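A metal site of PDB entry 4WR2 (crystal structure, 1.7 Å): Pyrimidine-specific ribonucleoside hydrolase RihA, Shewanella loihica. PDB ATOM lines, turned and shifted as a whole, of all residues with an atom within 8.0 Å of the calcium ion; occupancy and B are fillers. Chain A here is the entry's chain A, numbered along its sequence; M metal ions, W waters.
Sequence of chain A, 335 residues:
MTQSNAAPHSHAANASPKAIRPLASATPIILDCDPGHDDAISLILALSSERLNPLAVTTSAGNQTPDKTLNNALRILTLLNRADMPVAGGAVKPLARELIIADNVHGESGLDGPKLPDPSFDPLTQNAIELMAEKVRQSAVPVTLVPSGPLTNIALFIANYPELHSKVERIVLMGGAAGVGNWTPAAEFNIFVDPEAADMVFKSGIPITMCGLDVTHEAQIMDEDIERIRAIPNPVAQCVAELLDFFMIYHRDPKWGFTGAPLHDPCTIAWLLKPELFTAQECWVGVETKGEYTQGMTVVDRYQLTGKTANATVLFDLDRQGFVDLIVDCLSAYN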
ATOM      1  N   ASP A  32      18.842  23.657 -15.126  1.00  0.00           N
ATOM      2  CA  ASP A  32      18.102  23.283 -16.319  1.00  0.00           C
ATOM      3  C   ASP A  32      18.724  22.000 -16.812  1.00  0.00           C
ATOM      4  O   ASP A  32      19.923  21.960 -17.075  1.00  0.00           O
ATOM      5  CB  ASP A  32      18.153  24.397 -17.363  1.00  0.00           C
ATOM      6  CG  ASP A  32      17.404  24.076 -18.624  1.00  0.00           C
ATOM      7  OD1 ASP A  32      16.152  24.135 -18.641  1.00  0.00           O
ATOM      8  OD2 ASP A  32      18.076  23.778 -19.645  1.00  0.00           O
ATOM      9  N   CYS A  33      17.957  20.927 -16.854  1.00  0.00           N
ATOM     10  CA  CYS A  33      18.557  19.598 -16.931  1.00  0.00           C
ATOM     11  C   CYS A  33      17.692  18.603 -17.704  1.00  0.00           C
ATOM     12  O   CYS A  33      16.484  18.780 -17.806  1.00  0.00           O
ATOM     13  CB  CYS A  33      18.861  19.069 -15.521  1.00  0.00           C
ATOM     14  SG  CYS A  33      17.468  18.998 -14.410  1.00  0.00           S
ATOM     15  N   ASP A  34      18.315  17.530 -18.174  1.00  0.00           N
ATOM     16  CA  ASP A  34      17.582  16.490 -18.875  1.00  0.00           C
ATOM     17  C   ASP A  34      17.876  15.144 -18.230  1.00  0.00           C
ATOM     18  O   ASP A  34      18.438  14.242 -18.851  1.00  0.00           O
ATOM     19  CB  ASP A  34      17.952  16.489 -20.386  1.00  0.00           C
ATOM     20  CG  ASP A  34      19.432  16.136 -20.657  1.00  0.00           C
ATOM     21  OD1 ASP A  34      20.296  16.484 -19.837  1.00  0.00           O
ATOM     22  OD2 ASP A  34      19.724  15.524 -21.726  1.00  0.00           O
ATOM     23  N   PRO A  35      17.465  14.990 -16.955  1.00  0.00           N
ATOM     24  CA  PRO A  35      18.021  13.785 -16.328  1.00  0.00           C
ATOM     25  C   PRO A  35      17.585  12.458 -16.842  1.00  0.00           C
ATOM     26  O   PRO A  35      16.323  12.358 -17.097  1.00  0.00           O
ATOM     27  CB  PRO A  35      17.528  13.883 -14.885  1.00  0.00           C
ATOM     28  CG  PRO A  35      16.840  15.187 -14.780  1.00  0.00           C
ATOM     29  CD  PRO A  35      16.402  15.542 -16.121  1.00  0.00           C
ATOM     30  N   GLY A  36      18.636  11.756 -17.311  1.00  0.00           N
ATOM     31  CA  GLY A  36      19.220  10.630 -16.743  1.00  0.00           C
ATOM     32  C   GLY A  36      20.218  10.963 -15.629  1.00  0.00           C
ATOM     33  O   GLY A  36      20.057  11.859 -14.805  1.00  0.00           O
ATOM     34  N   HIS A  37      21.261  10.168 -15.573  1.00  0.00           N
ATOM     35  CA  HIS A  37      21.848   9.865 -14.274  1.00  0.00           C
ATOM     36  C   HIS A  37      22.933  10.842 -13.891  1.00  0.00           C
ATOM     37  O   HIS A  37      23.101  11.171 -12.716  1.00  0.00           O
ATOM     38  CB  HIS A  37      22.405   8.442 -14.300  1.00  0.00           C
ATOM     39  CG  HIS A  37      21.352   7.391 -14.455  1.00  0.00           C
ATOM     40  ND1 HIS A  37      21.459   6.358 -15.358  1.00  0.00           N
ATOM     41  CD2 HIS A  37      20.172   7.210 -13.803  1.00  0.00           C
ATOM     42  CE1 HIS A  37      20.392   5.577 -15.254  1.00  0.00           C
ATOM     43  NE2 HIS A  37      19.605   6.069 -14.316  1.00  0.00           N
ATOM     44  N   ASP A  38      23.673  11.323 -14.895  1.00  0.00           N
ATOM     45  CA  ASP A  38      24.655  12.381 -14.667  1.00  0.00           C
ATOM     46  C   ASP A  38      23.990  13.613 -14.085  1.00  0.00           C
ATOM     47  O   ASP A  38      24.480  14.198 -13.120  1.00  0.00           O
ATOM     48  CB  ASP A  38      25.370  12.747 -15.976  1.00  0.00           C
ATOM     49  CG  ASP A  38      26.721  12.125 -16.099  1.00  0.00           C
ATOM     50  OD1 ASP A  38      27.645  12.560 -15.381  1.00  0.00           O
ATOM     51  OD2 ASP A  38      26.865  11.191 -16.911  1.00  0.00           O
ATOM     52  N   ASP A  39      22.868  14.010 -14.677  1.00  0.00           N
ATOM     53  CA  ASP A  39      22.138  15.165 -14.163  1.00  0.00           C
ATOM     54  C   ASP A  39      21.679  14.927 -12.751  1.00  0.00           C
ATOM     55  O   ASP A  39      21.624  15.850 -11.942  1.00  0.00           O
ATOM     56  CB  ASP A  39      20.903  15.521 -15.011  1.00  0.00           C
ATOM     57  CG  ASP A  39      21.203  15.662 -16.483  1.00  0.00           C
ATOM     58  OD1 ASP A  39      21.477  14.632 -17.099  1.00  0.00           O
ATOM     59  OD2 ASP A  39      21.143  16.811 -17.012  1.00  0.00           O
ATOM     60  N   ALA A  40      21.266  13.686 -12.466  1.00  0.00           N
ATOM     61  CA  ALA A  40      20.795  13.368 -11.130  1.00  0.00           C
ATOM     62  C   ALA A  40      21.881  13.663 -10.092  1.00  0.00           C
ATOM     63  O   ALA A  40      21.603  14.258  -9.045  1.00  0.00           O
ATOM     64  CB  ALA A  40      20.370  11.912 -11.051  1.00  0.00           C
ATOM     65  N   SER A  42      24.377  15.703 -10.433  1.00  0.00           N
ATOM     66  CA  SER A  42      24.481  17.162 -10.391  1.00  0.00           C
ATOM     67  C   SER A  42      23.448  17.819  -9.486  1.00  0.00           C
ATOM     68  O   SER A  42      23.803  18.677  -8.647  1.00  0.00           O
ATOM     69  CB  SER A  42      24.347  17.721 -11.817  1.00  0.00           C
ATOM     70  OG  SER A  42      25.355  18.638 -12.031  1.00  0.00           O
ATOM     71  N   SER A  60      14.940  20.020 -19.827  1.00  0.00           N
ATOM     72  CA  SER A  60      15.165  19.950 -21.262  1.00  0.00           C
ATOM     73  C   SER A  60      15.090  18.502 -21.729  1.00  0.00           C
ATOM     74  O   SER A  60      14.936  17.595 -20.909  1.00  0.00           O
ATOM     75  CB  SER A  60      16.517  20.553 -21.605  1.00  0.00           C
ATOM     76  OG  SER A  60      17.590  19.863 -20.939  1.00  0.00           O
ATOM     77  N   ASN A  63      17.690  12.872 -25.593  1.00  0.00           N
ATOM     78  CA  ASN A  63      17.500  11.541 -26.170  1.00  0.00           C
ATOM     79  C   ASN A  63      16.444  10.740 -25.429  1.00  0.00           C
ATOM     80  O   ASN A  63      16.355   9.524 -25.582  1.00  0.00           O
ATOM     81  CB  ASN A  63      18.832  10.768 -26.204  1.00  0.00           C
ATOM     82  CG  ASN A  63      19.405  10.511 -24.823  1.00  0.00           C
ATOM     83  OD1 ASN A  63      18.956  11.047 -23.819  1.00  0.00           O
ATOM     84  ND2 ASN A  63      20.418   9.654 -24.785  1.00  0.00           N
ATOM     85  N   PRO A 147      22.774  24.933 -17.076  1.00  0.00           N
ATOM     86  CA  PRO A 147      22.205  23.888 -17.908  1.00  0.00           C
ATOM     87  C   PRO A 147      23.105  22.682 -18.004  1.00  0.00           C
ATOM     88  O   PRO A 147      24.307  22.840 -18.077  1.00  0.00           O
ATOM     89  CB  PRO A 147      22.029  24.563 -19.261  1.00  0.00           C
ATOM     90  CG  PRO A 147      23.065  25.600 -19.291  1.00  0.00           C
ATOM     91  CD  PRO A 147      23.245  26.075 -17.872  1.00  0.00           C
ATOM     92  N   SER A 148      22.506  21.484 -18.052  1.00  0.00           N
ATOM     93  CA  SER A 148      23.307  20.273 -18.204  1.00  0.00           C
ATOM     94  C   SER A 148      22.737  19.354 -19.282  1.00  0.00           C
ATOM     95  O   SER A 148      23.143  18.197 -19.378  1.00  0.00           O
ATOM     96  CB  SER A 148      23.389  19.532 -16.853  1.00  0.00           C
ATOM     97  OG  SER A 148      22.089  19.251 -16.347  1.00  0.00           O
ATOM     98  N   GLY A 149      21.835  19.892 -20.090  1.00  0.00           N
ATOM     99  CA  GLY A 149      21.319  19.197 -21.268  1.00  0.00           C
ATOM    100  C   GLY A 149      21.372  20.119 -22.460  1.00  0.00           C
ATOM    101  O   GLY A 149      22.104  21.121 -22.436  1.00  0.00           O
ATOM    102  N   PRO A 150      20.619  19.798 -23.507  1.00  0.00           N
ATOM    103  CA  PRO A 150      20.547  20.701 -24.663  1.00  0.00           C
ATOM    104  C   PRO A 150      20.134  22.096 -24.210  1.00  0.00           C
ATOM    105  O   PRO A 150      19.424  22.236 -23.220  1.00  0.00           O
ATOM    106  CB  PRO A 150      19.478  20.045 -25.549  1.00  0.00           C
ATOM    107  CG  PRO A 150      19.579  18.575 -25.199  1.00  0.00           C
ATOM    108  CD  PRO A 150      19.792  18.585 -23.700  1.00  0.00           C
ATOM    109  N   MET A 174      27.199  22.297 -19.122  1.00  0.00           N
ATOM    110  CA  MET A 174      27.944  21.093 -19.499  1.00  0.00           C
ATOM    111  C   MET A 174      27.636  20.883 -20.981  1.00  0.00           C
ATOM    112  O   MET A 174      26.483  20.718 -21.392  1.00  0.00           O
ATOM    113  CB  MET A 174      27.556  19.811 -18.707  1.00  0.00           C
ATOM    114  CG  MET A 174      28.609  18.635 -18.861  1.00  0.00           C
ATOM    115  SD  MET A 174      28.189  17.723 -20.545  1.00  0.00           S
ATOM    116  CE  MET A 174      30.038  17.583 -21.227  1.00  0.00           C
ATOM    117  N   GLU A 188      29.881  17.134 -29.387  1.00  0.00           N
ATOM    118  CA  GLU A 188      29.373  16.617 -28.135  1.00  0.00           C
ATOM    119  C   GLU A 188      27.837  16.591 -28.159  1.00  0.00           C
ATOM    120  O   GLU A 188      27.190  17.430 -28.803  1.00  0.00           O
ATOM    121  CB  GLU A 188      29.929  17.449 -26.984  1.00  0.00           C
ATOM    122  CG  GLU A 188      29.472  17.021 -25.585  1.00  0.00           C
ATOM    123  CD  GLU A 188      28.106  17.569 -25.219  1.00  0.00           C
ATOM    124  OE1 GLU A 188      27.779  18.708 -25.658  1.00  0.00           O
ATOM    125  OE2 GLU A 188      27.360  16.872 -24.456  1.00  0.00           O
ATOM    126  N   PHE A 189      27.262  15.637 -27.446  1.00  0.00           N
ATOM    127  CA  PHE A 189      25.820  15.368 -27.496  1.00  0.00           C
ATOM    128  C   PHE A 189      24.896  16.553 -27.209  1.00  0.00           C
ATOM    129  O   PHE A 189      23.998  16.855 -28.026  1.00  0.00           O
ATOM    130  CB  PHE A 189      25.496  14.234 -26.525  1.00  0.00           C
ATOM    131  CG  PHE A 189      24.040  13.918 -26.422  1.00  0.00           C
ATOM    132  CD1 PHE A 189      23.413  13.165 -27.389  1.00  0.00           C
ATOM    133  CD2 PHE A 189      23.289  14.406 -25.344  1.00  0.00           C
ATOM    134  CE1 PHE A 189      22.034  12.878 -27.285  1.00  0.00           C
ATOM    135  CE2 PHE A 189      21.944  14.126 -25.241  1.00  0.00           C
ATOM    136  CZ  PHE A 189      21.320  13.360 -26.215  1.00  0.00           C
ATOM    137  N   ASN A 190      25.073  17.235 -26.082  1.00  0.00           N
ATOM    138  CA  ASN A 190      24.165  18.331 -25.737  1.00  0.00           C
ATOM    139  C   ASN A 190      24.115  19.417 -26.803  1.00  0.00           C
ATOM    140  O   ASN A 190      23.052  19.969 -27.102  1.00  0.00           O
ATOM    141  CB  ASN A 190      24.555  18.977 -24.418  1.00  0.00           C
ATOM    142  CG  ASN A 190      24.208  18.131 -23.228  1.00  0.00           C
ATOM    143  OD1 ASN A 190      23.415  17.173 -23.319  1.00  0.00           O
ATOM    144  ND2 ASN A 190      24.795  18.472 -22.112  1.00  0.00           N
ATOM    145  N   HIS A 264      30.091  13.848 -15.935  1.00  0.00           N
ATOM    146  CA  HIS A 264      30.052  15.027 -16.768  1.00  0.00           C
ATOM    147  C   HIS A 264      29.387  16.196 -16.055  1.00  0.00           C
ATOM    148  O   HIS A 264      30.058  17.135 -15.601  1.00  0.00           O
ATOM    149  CB  HIS A 264      29.349  14.732 -18.105  1.00  0.00           C
ATOM    150  CG  HIS A 264      29.952  13.585 -18.850  1.00  0.00           C
ATOM    151  ND1 HIS A 264      31.023  13.741 -19.707  1.00  0.00           N
ATOM    152  CD2 HIS A 264      29.649  12.264 -18.850  1.00  0.00           C
ATOM    153  CE1 HIS A 264      31.347  12.559 -20.214  1.00  0.00           C
ATOM    154  NE2 HIS A 264      30.534  11.654 -19.706  1.00  0.00           N
ATOM    155  N   ASP A 265      28.062  16.139 -15.958  1.00  0.00           N
ATOM    156  CA  ASP A 265      27.272  17.270 -15.473  1.00  0.00           C
ATOM    157  C   ASP A 265      27.735  17.800 -14.107  1.00  0.00           C
ATOM    158  O   ASP A 265      27.782  19.022 -13.896  1.00  0.00           O
ATOM    159  CB  ASP A 265      25.799  16.911 -15.450  1.00  0.00           C
ATOM    160  CG  ASP A 265      25.276  16.487 -16.822  1.00  0.00           C
ATOM    161  OD1 ASP A 265      26.058  16.510 -17.781  1.00  0.00           O
ATOM    162  OD2 ASP A 265      24.102  16.116 -16.963  1.00  0.00           O
ATOM    163  N   PRO A 266      28.118  16.917 -13.169  1.00  0.00           N
ATOM    164  CA  PRO A 266      28.537  17.428 -11.860  1.00  0.00           C
ATOM    165  C   PRO A 266      29.726  18.391 -11.898  1.00  0.00           C
ATOM    166  O   PRO A 266      29.928  19.127 -10.931  1.00  0.00           O
ATOM    167  CB  PRO A 266      28.890  16.156 -11.084  1.00  0.00           C
ATOM    168  CG  PRO A 266      27.935  15.160 -11.649  1.00  0.00           C
ATOM    169  CD  PRO A 266      27.969  15.453 -13.140  1.00  0.00           C
HETATM  170 CA    CA M   1      22.579  15.957 -18.996  1.00  0.00          CA
HETATM  171  O   HOH W   1      24.965  15.878 -20.019  1.00  0.00           O
HETATM  172  O   HOH W   2      21.156  13.499 -19.609  1.00  0.00           O
HETATM  173  O   HOH W   3      22.458  15.472 -21.508  1.00  0.00           O
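Water W3 lies within hydrogen-bond range of OD1 of Asn 190 (2.7 Å) and OD2 of Asp 34 (2.7 Å). Water W1 lies within hydrogen-bond range of OD1 of Asp 265, ND2 of Asn 190 and SD of Met 174.
ND2 of Asn 190 sits close to O of Ser 148 (3.2 Å). O of Asp 265 is in hydrogen-bond range of OG of Ser 42, at 3.1 Å. N of Ser 148 is in hydrogen-bond range of O of Asp 32.
Within 4 Å of the calcium ion: Asp 34, Asp 39, Ser 148 and Asp 265.
The calcium ion is bound by O of Ser 148, OD1 of Asp 34, OD2 of Asp 265, water W3, OD1 of Asp 39, OD2 of Asp 39 and water W1. The calcium ion has seven donor atoms within binding distance. Slightly farther from the calcium ion lies water W2 (2.9 Å).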
